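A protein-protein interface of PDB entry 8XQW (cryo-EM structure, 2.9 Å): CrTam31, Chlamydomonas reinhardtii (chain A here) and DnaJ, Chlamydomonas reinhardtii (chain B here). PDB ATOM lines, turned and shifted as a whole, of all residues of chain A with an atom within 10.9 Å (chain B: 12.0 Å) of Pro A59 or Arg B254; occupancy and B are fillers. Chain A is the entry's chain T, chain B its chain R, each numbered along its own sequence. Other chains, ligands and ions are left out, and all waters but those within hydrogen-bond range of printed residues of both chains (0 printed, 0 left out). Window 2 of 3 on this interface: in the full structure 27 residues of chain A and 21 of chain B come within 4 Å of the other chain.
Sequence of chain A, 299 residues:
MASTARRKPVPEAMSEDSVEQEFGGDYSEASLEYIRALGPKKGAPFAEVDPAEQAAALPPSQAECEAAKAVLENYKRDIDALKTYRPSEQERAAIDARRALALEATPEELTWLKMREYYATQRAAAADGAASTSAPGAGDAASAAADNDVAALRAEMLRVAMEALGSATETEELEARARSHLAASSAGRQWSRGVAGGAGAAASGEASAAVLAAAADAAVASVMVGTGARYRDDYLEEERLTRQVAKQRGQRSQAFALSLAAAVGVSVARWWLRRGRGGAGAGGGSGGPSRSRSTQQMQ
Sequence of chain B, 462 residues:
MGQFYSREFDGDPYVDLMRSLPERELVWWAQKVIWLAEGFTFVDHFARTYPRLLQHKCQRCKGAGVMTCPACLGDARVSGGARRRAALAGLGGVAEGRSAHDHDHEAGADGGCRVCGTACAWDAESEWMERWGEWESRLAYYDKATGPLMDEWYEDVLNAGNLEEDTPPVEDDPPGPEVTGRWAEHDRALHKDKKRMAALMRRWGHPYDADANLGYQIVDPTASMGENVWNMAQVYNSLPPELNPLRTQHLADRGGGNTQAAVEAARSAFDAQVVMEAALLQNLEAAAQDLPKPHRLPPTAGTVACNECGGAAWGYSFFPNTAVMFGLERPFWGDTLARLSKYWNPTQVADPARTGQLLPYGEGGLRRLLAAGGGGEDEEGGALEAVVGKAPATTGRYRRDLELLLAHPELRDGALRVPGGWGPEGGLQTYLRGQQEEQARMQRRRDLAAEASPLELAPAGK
The backbone carbonyl oxygen of Ala A56 lies within hydrogen-bond range of the backbone NH of Gly B256, 3.2 Å away.
The side-chain carboxylate (OD2) of Asp B253 is in salt-bridge range of the guanidinium group (NH2) of Arg B254.
Among the printed residues, merely in contact across the chains: Pro A59 with Arg B254 (3.1 Å), Ala A56 with Gly B255 (3.2 Å), Gln A54 with Leu B251 (3.2 Å), Glu A53 with Thr B259 (3.3 Å), Ala A57 with Leu B251 (3.6 Å) and Leu A58 with Gly B255 (3.7 Å).
Printed residues of chain B within 4 Å of Glu A53: Thr B259 (3.3 Å).
Of the printed residues of chain B, Gln A54 touches Leu B251 (3.2 Å).
Ala A56 touches two residues of chain B.
Of the printed residues of chain B, Ala A57 touches Leu B251.
Of the printed residues of chain B, Leu A58 touches Gly B255 (3.7 Å).
Pro A59 touches just one residue of chain B: Arg B254.
Of the printed residues of chain A, Leu B251 touches Gln A54 (3.2 Å) and Ala A57 (3.6 Å).
Printed residues of chain A within 4 Å of Arg B254: Pro A59.
Gly B255 touches just these residues of chain A: Ala A56 and Leu A58.
Gly B256 touches just one residue of chain A: Ala A56 (3.2 Å).
Of the printed residues of chain A, Thr B259 touches Glu A53 (3.3 Å).
Of the 14 printed residues of chain B, 5 touch a printed residue of chain A.
Printed residues of chain B that touch a printed residue of chain A: Leu B251, Arg B254, Gly B255, Gly B256 and Thr B259.
Hydrophobic or aromatic side chains of chain B within 4 Å of the printed part of chain A: Leu B251.
Of the 13 printed residues of chain A, 6 touch a printed residue of chain B.
Hydrophobic or aromatic side chains of chain A that line the printed part of chain B: Ala A57 and Pro A59.
Among the printed residues, 7 pairs touch across the chains.
Among the printed residues, no Asp or Glu carboxylate lies within 4 Å of a Lys or Arg side-chain nitrogen of the other chain.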
ATOM      1  N   GLU A  53     -19.184 -14.050 -11.494  1.00  0.00           N
ATOM      2  CA  GLU A  53     -19.483 -14.989 -12.566  1.00  0.00           C
ATOM      3  C   GLU A  53     -20.726 -14.586 -13.338  1.00  0.00           C
ATOM      4  O   GLU A  53     -20.714 -14.615 -14.572  1.00  0.00           O
ATOM      5  CB  GLU A  53     -19.682 -16.393 -11.994  1.00  0.00           C
ATOM      6  CG  GLU A  53     -19.507 -17.533 -12.983  1.00  0.00           C
ATOM      7  CD  GLU A  53     -19.216 -18.860 -12.298  1.00  0.00           C
ATOM      8  OE1 GLU A  53     -19.418 -19.917 -12.932  1.00  0.00           O
ATOM      9  OE2 GLU A  53     -18.792 -18.850 -11.124  1.00  0.00           O
ATOM     10  N   GLN A  54     -21.788 -14.202 -12.628  1.00  0.00           N
ATOM     11  CA  GLN A  54     -23.039 -13.829 -13.277  1.00  0.00           C
ATOM     12  C   GLN A  54     -22.909 -12.501 -14.008  1.00  0.00           C
ATOM     13  O   GLN A  54     -23.529 -12.298 -15.058  1.00  0.00           O
ATOM     14  CB  GLN A  54     -24.156 -13.764 -12.239  1.00  0.00           C
ATOM     15  CG  GLN A  54     -25.519 -13.495 -12.816  1.00  0.00           C
ATOM     16  CD  GLN A  54     -26.112 -14.716 -13.476  1.00  0.00           C
ATOM     17  OE1 GLN A  54     -26.892 -15.450 -12.868  1.00  0.00           O
ATOM     18  NE2 GLN A  54     -25.745 -14.947 -14.731  1.00  0.00           N
ATOM     19  N   ALA A  55     -22.089 -11.593 -13.481  1.00  0.00           N
ATOM     20  CA  ALA A  55     -21.926 -10.265 -14.052  1.00  0.00           C
ATOM     21  C   ALA A  55     -21.300 -10.278 -15.439  1.00  0.00           C
ATOM     22  O   ALA A  55     -21.149  -9.206 -16.033  1.00  0.00           O
ATOM     23  CB  ALA A  55     -21.084  -9.400 -13.116  1.00  0.00           C
ATOM     24  N   ALA A  56     -20.924 -11.441 -15.965  1.00  0.00           N
ATOM     25  CA  ALA A  56     -20.350 -11.520 -17.299  1.00  0.00           C
ATOM     26  C   ALA A  56     -21.338 -12.014 -18.342  1.00  0.00           C
ATOM     27  O   ALA A  56     -21.136 -11.763 -19.533  1.00  0.00           O
ATOM     28  CB  ALA A  56     -19.120 -12.432 -17.291  1.00  0.00           C
ATOM     29  N   ALA A  57     -22.398 -12.702 -17.929  1.00  0.00           N
ATOM     30  CA  ALA A  57     -23.364 -13.262 -18.865  1.00  0.00           C
ATOM     31  C   ALA A  57     -24.260 -12.213 -19.511  1.00  0.00           C
ATOM     32  O   ALA A  57     -25.107 -12.572 -20.336  1.00  0.00           O
ATOM     33  CB  ALA A  57     -24.226 -14.308 -18.157  1.00  0.00           C
ATOM     34  N   LEU A  58     -24.096 -10.939 -19.172  1.00  0.00           N
ATOM     35  CA  LEU A  58     -25.010  -9.951 -19.719  1.00  0.00           C
ATOM     36  C   LEU A  58     -24.372  -9.192 -20.880  1.00  0.00           C
ATOM     37  O   LEU A  58     -23.175  -8.884 -20.851  1.00  0.00           O
ATOM     38  CB  LEU A  58     -25.452  -8.970 -18.629  1.00  0.00           C
ATOM     39  CG  LEU A  58     -24.466  -7.933 -18.098  1.00  0.00           C
ATOM     40  CD1 LEU A  58     -24.746  -6.549 -18.674  1.00  0.00           C
ATOM     41  CD2 LEU A  58     -24.498  -7.904 -16.581  1.00  0.00           C
ATOM     42  N   PRO A  59     -25.158  -8.888 -21.910  1.00  0.00           N
ATOM     43  CA  PRO A  59     -24.607  -8.279 -23.119  1.00  0.00           C
ATOM     44  C   PRO A  59     -24.472  -6.779 -22.950  1.00  0.00           C
ATOM     45  O   PRO A  59     -24.893  -6.228 -21.922  1.00  0.00           O
ATOM     46  CB  PRO A  59     -25.660  -8.623 -24.182  1.00  0.00           C
ATOM     47  CG  PRO A  59     -26.936  -8.583 -23.427  1.00  0.00           C
ATOM     48  CD  PRO A  59     -26.616  -9.072 -22.013  1.00  0.00           C
ATOM     49  N   PRO A  60     -23.900  -6.077 -23.926  1.00  0.00           N
ATOM     50  CA  PRO A  60     -23.854  -4.616 -23.834  1.00  0.00           C
ATOM     51  C   PRO A  60     -25.255  -4.032 -23.811  1.00  0.00           C
ATOM     52  O   PRO A  60     -26.147  -4.454 -24.553  1.00  0.00           O
ATOM     53  CB  PRO A  60     -23.090  -4.197 -25.097  1.00  0.00           C
ATOM     54  CG  PRO A  60     -23.203  -5.362 -26.018  1.00  0.00           C
ATOM     55  CD  PRO A  60     -23.198  -6.563 -25.127  1.00  0.00           C
ATOM     56  N   SER A  61     -25.444  -3.054 -22.931  1.00  0.00           N
ATOM     57  CA  SER A  61     -26.742  -2.432 -22.734  1.00  0.00           C
ATOM     58  C   SER A  61     -26.926  -1.300 -23.743  1.00  0.00           C
ATOM     59  O   SER A  61     -26.110  -1.101 -24.646  1.00  0.00           O
ATOM     60  CB  SER A  61     -26.886  -1.952 -21.291  1.00  0.00           C
ATOM     61  OG  SER A  61     -26.411  -2.924 -20.375  1.00  0.00           O
ATOM     62  N   GLN A  62     -28.005  -0.533 -23.580  1.00  0.00           N
ATOM     63  CA  GLN A  62     -28.440   0.366 -24.642  1.00  0.00           C
ATOM     64  C   GLN A  62     -27.530   1.579 -24.794  1.00  0.00           C
ATOM     65  O   GLN A  62     -27.512   2.194 -25.860  1.00  0.00           O
ATOM     66  CB  GLN A  62     -29.879   0.812 -24.390  1.00  0.00           C
ATOM     67  CG  GLN A  62     -30.838  -0.349 -24.214  1.00  0.00           C
ATOM     68  CD  GLN A  62     -30.524  -1.505 -25.149  1.00  0.00           C
ATOM     69  OE1 GLN A  62     -29.997  -2.536 -24.729  1.00  0.00           O
ATOM     70  NE2 GLN A  62     -30.849  -1.337 -26.427  1.00  0.00           N
ATOM     71  N   ALA A  63     -26.776   1.940 -23.755  1.00  0.00           N
ATOM     72  CA  ALA A  63     -25.872   3.082 -23.872  1.00  0.00           C
ATOM     73  C   ALA A  63     -24.817   2.835 -24.941  1.00  0.00           C
ATOM     74  O   ALA A  63     -24.632   3.649 -25.855  1.00  0.00           O
ATOM     75  CB  ALA A  63     -25.213   3.368 -22.524  1.00  0.00           C
ATOM     76  N   GLU A  64     -24.111   1.709 -24.842  1.00  0.00           N
ATOM     77  CA  GLU A  64     -23.070   1.399 -25.813  1.00  0.00           C
ATOM     78  C   GLU A  64     -23.662   1.149 -27.195  1.00  0.00           C
ATOM     79  O   GLU A  64     -23.075   1.537 -28.208  1.00  0.00           O
ATOM     80  CB  GLU A  64     -22.261   0.189 -25.343  1.00  0.00           C
ATOM     81  CG  GLU A  64     -21.446   0.444 -24.082  1.00  0.00           C
ATOM     82  CD  GLU A  64     -20.993  -0.832 -23.400  1.00  0.00           C
ATOM     83  OE1 GLU A  64     -21.020  -0.875 -22.153  1.00  0.00           O
ATOM     84  OE2 GLU A  64     -20.605  -1.787 -24.107  1.00  0.00           O
ATOM     85  N   CYS A  65     -24.833   0.513 -27.253  1.00  0.00           N
ATOM     86  CA  CYS A  65     -25.474   0.239 -28.533  1.00  0.00           C
ATOM     87  C   CYS A  65     -25.883   1.529 -29.234  1.00  0.00           C
ATOM     88  O   CYS A  65     -25.722   1.671 -30.449  1.00  0.00           O
ATOM     89  CB  CYS A  65     -26.680  -0.674 -28.318  1.00  0.00           C
ATOM     90  SG  CYS A  65     -26.263  -2.266 -27.575  1.00  0.00           S
ATOM     91  N   THR B 248     -22.790 -24.931 -14.752  1.00  0.00           N
ATOM     92  CA  THR B 248     -22.635 -23.806 -15.665  1.00  0.00           C
ATOM     93  C   THR B 248     -23.240 -24.063 -17.041  1.00  0.00           C
ATOM     94  O   THR B 248     -23.286 -23.144 -17.867  1.00  0.00           O
ATOM     95  CB  THR B 248     -21.149 -23.459 -15.802  1.00  0.00           C
ATOM     96  OG1 THR B 248     -20.514 -23.586 -14.524  1.00  0.00           O
ATOM     97  CG2 THR B 248     -20.966 -22.033 -16.293  1.00  0.00           C
ATOM     98  N   GLN B 249     -23.727 -25.276 -17.312  1.00  0.00           N
ATOM     99  CA  GLN B 249     -24.116 -25.618 -18.678  1.00  0.00           C
ATOM    100  C   GLN B 249     -25.277 -24.788 -19.212  1.00  0.00           C
ATOM    101  O   GLN B 249     -25.665 -24.979 -20.370  1.00  0.00           O
ATOM    102  CB  GLN B 249     -24.467 -27.105 -18.781  1.00  0.00           C
ATOM    103  CG  GLN B 249     -25.369 -27.645 -17.678  1.00  0.00           C
ATOM    104  CD  GLN B 249     -26.739 -26.997 -17.629  1.00  0.00           C
ATOM    105  OE1 GLN B 249     -27.585 -27.241 -18.488  1.00  0.00           O
ATOM    106  NE2 GLN B 249     -26.966 -26.167 -16.618  1.00  0.00           N
ATOM    107  N   HIS B 250     -25.851 -23.881 -18.420  1.00  0.00           N
ATOM    108  CA  HIS B 250     -27.051 -23.197 -18.882  1.00  0.00           C
ATOM    109  C   HIS B 250     -26.797 -21.796 -19.427  1.00  0.00           C
ATOM    110  O   HIS B 250     -27.416 -21.428 -20.429  1.00  0.00           O
ATOM    111  CB  HIS B 250     -28.106 -23.149 -17.769  1.00  0.00           C
ATOM    112  CG  HIS B 250     -27.743 -22.278 -16.613  1.00  0.00           C
ATOM    113  ND1 HIS B 250     -27.079 -22.755 -15.504  1.00  0.00           N
ATOM    114  CD2 HIS B 250     -27.969 -20.965 -16.378  1.00  0.00           C
ATOM    115  CE1 HIS B 250     -26.899 -21.770 -14.643  1.00  0.00           C
ATOM    116  NE2 HIS B 250     -27.434 -20.675 -15.148  1.00  0.00           N
ATOM    117  N   LEU B 251     -25.911 -21.005 -18.828  1.00  0.00           N
ATOM    118  CA  LEU B 251     -25.666 -19.656 -19.331  1.00  0.00           C
ATOM    119  C   LEU B 251     -24.199 -19.482 -19.686  1.00  0.00           C
ATOM    120  O   LEU B 251     -23.328 -19.556 -18.814  1.00  0.00           O
ATOM    121  CB  LEU B 251     -26.125 -18.586 -18.331  1.00  0.00           C
ATOM    122  CG  LEU B 251     -25.629 -18.412 -16.891  1.00  0.00           C
ATOM    123  CD1 LEU B 251     -24.333 -17.616 -16.791  1.00  0.00           C
ATOM    124  CD2 LEU B 251     -26.714 -17.730 -16.082  1.00  0.00           C
ATOM    125  N   ALA B 252     -23.931 -19.300 -20.978  1.00  0.00           N
ATOM    126  CA  ALA B 252     -22.646 -18.818 -21.468  1.00  0.00           C
ATOM    127  C   ALA B 252     -22.806 -18.348 -22.906  1.00  0.00           C
ATOM    128  O   ALA B 252     -23.045 -19.161 -23.803  1.00  0.00           O
ATOM    129  CB  ALA B 252     -21.573 -19.903 -21.383  1.00  0.00           C
ATOM    130  N   ASP B 253     -22.661 -17.054 -23.143  1.00  0.00           N
ATOM    131  CA  ASP B 253     -22.854 -16.490 -24.476  1.00  0.00           C
ATOM    132  C   ASP B 253     -22.191 -15.117 -24.517  1.00  0.00           C
ATOM    133  O   ASP B 253     -21.356 -14.786 -23.665  1.00  0.00           O
ATOM    134  CB  ASP B 253     -24.335 -16.463 -24.870  1.00  0.00           C
ATOM    135  CG  ASP B 253     -25.263 -16.288 -23.686  1.00  0.00           C
ATOM    136  OD1 ASP B 253     -24.780 -16.235 -22.537  1.00  0.00           O
ATOM    137  OD2 ASP B 253     -26.489 -16.203 -23.914  1.00  0.00           O
ATOM    138  N   ARG B 254     -22.581 -14.323 -25.523  1.00  0.00           N
ATOM    139  CA  ARG B 254     -21.797 -13.194 -26.034  1.00  0.00           C
ATOM    140  C   ARG B 254     -21.139 -12.345 -24.950  1.00  0.00           C
ATOM    141  O   ARG B 254     -20.129 -11.681 -25.212  1.00  0.00           O
ATOM    142  CB  ARG B 254     -22.698 -12.308 -26.893  1.00  0.00           C
ATOM    143  CG  ARG B 254     -23.674 -11.472 -26.089  1.00  0.00           C
ATOM    144  CD  ARG B 254     -25.091 -11.624 -26.600  1.00  0.00           C
ATOM    145  NE  ARG B 254     -25.779 -12.763 -26.005  1.00  0.00           N
ATOM    146  CZ  ARG B 254     -26.350 -12.750 -24.802  1.00  0.00           C
ATOM    147  NH1 ARG B 254     -26.286 -11.665 -24.051  1.00  0.00           N
ATOM    148  NH2 ARG B 254     -26.972 -13.826 -24.347  1.00  0.00           N
ATOM    149  N   GLY B 255     -21.709 -12.317 -23.746  1.00  0.00           N
ATOM    150  CA  GLY B 255     -21.243 -11.422 -22.703  1.00  0.00           C
ATOM    151  C   GLY B 255     -19.752 -11.478 -22.439  1.00  0.00           C
ATOM    152  O   GLY B 255     -19.040 -10.490 -22.639  1.00  0.00           O
ATOM    153  N   GLY B 256     -19.269 -12.630 -21.988  1.00  0.00           N
ATOM    154  CA  GLY B 256     -17.851 -12.810 -21.751  1.00  0.00           C
ATOM    155  C   GLY B 256     -17.233 -13.887 -22.617  1.00  0.00           C
ATOM    156  O   GLY B 256     -16.047 -13.815 -22.952  1.00  0.00           O
ATOM    157  N   GLY B 257     -18.029 -14.888 -22.991  1.00  0.00           N
ATOM    158  CA  GLY B 257     -17.506 -16.025 -23.727  1.00  0.00           C
ATOM    159  C   GLY B 257     -16.433 -16.792 -22.994  1.00  0.00           C
ATOM    160  O   GLY B 257     -15.561 -17.389 -23.629  1.00  0.00           O
ATOM    161  N   ASN B 258     -16.471 -16.795 -21.665  1.00  0.00           N
ATOM    162  CA  ASN B 258     -15.364 -17.300 -20.870  1.00  0.00           C
ATOM    163  C   ASN B 258     -15.751 -18.291 -19.790  1.00  0.00           C
ATOM    164  O   ASN B 258     -14.965 -19.206 -19.521  1.00  0.00           O
ATOM    165  CB  ASN B 258     -14.630 -16.132 -20.201  1.00  0.00           C
ATOM    166  CG  ASN B 258     -15.583 -15.106 -19.637  1.00  0.00           C
ATOM    167  OD1 ASN B 258     -16.798 -15.221 -19.798  1.00  0.00           O
ATOM    168  ND2 ASN B 258     -15.041 -14.094 -18.969  1.00  0.00           N
ATOM    169  N   THR B 259     -16.919 -18.151 -19.164  1.00  0.00           N
ATOM    170  CA  THR B 259     -17.195 -18.933 -17.965  1.00  0.00           C
ATOM    171  C   THR B 259     -17.158 -20.427 -18.244  1.00  0.00           C
ATOM    172  O   THR B 259     -16.556 -21.184 -17.475  1.00  0.00           O
ATOM    173  CB  THR B 259     -18.542 -18.530 -17.381  1.00  0.00           C
ATOM    174  OG1 THR B 259     -18.526 -17.129 -17.090  1.00  0.00           O
ATOM    175  CG2 THR B 259     -18.795 -19.288 -16.098  1.00  0.00           C
ATOM    176  N   GLN B 260     -17.766 -20.871 -19.336  1.00  0.00           N
ATOM    177  CA  GLN B 260     -17.691 -22.274 -19.710  1.00  0.00           C
ATOM    178  C   GLN B 260     -16.359 -22.640 -20.342  1.00  0.00           C
ATOM    179  O   GLN B 260     -16.079 -23.829 -20.513  1.00  0.00           O
ATOM    180  CB  GLN B 260     -18.824 -22.630 -20.670  1.00  0.00           C
ATOM    181  CG  GLN B 260     -20.155 -22.885 -19.989  1.00  0.00           C
ATOM    182  CD  GLN B 260     -21.168 -23.500 -20.928  1.00  0.00           C
ATOM    183  OE1 GLN B 260     -22.282 -23.831 -20.529  1.00  0.00           O
ATOM    184  NE2 GLN B 260     -20.783 -23.659 -22.188  1.00  0.00           N
ATOM    185  N   ALA B 261     -15.540 -21.653 -20.697  1.00  0.00           N
ATOM    186  CA  ALA B 261     -14.198 -21.914 -21.197  1.00  0.00           C
ATOM    187  C   ALA B 261     -13.185 -21.938 -20.064  1.00  0.00           C
ATOM    188  O   ALA B 261     -12.368 -22.858 -19.975  1.00  0.00           O
ATOM    189  CB  ALA B 261     -13.807 -20.862 -22.237  1.00  0.00           C
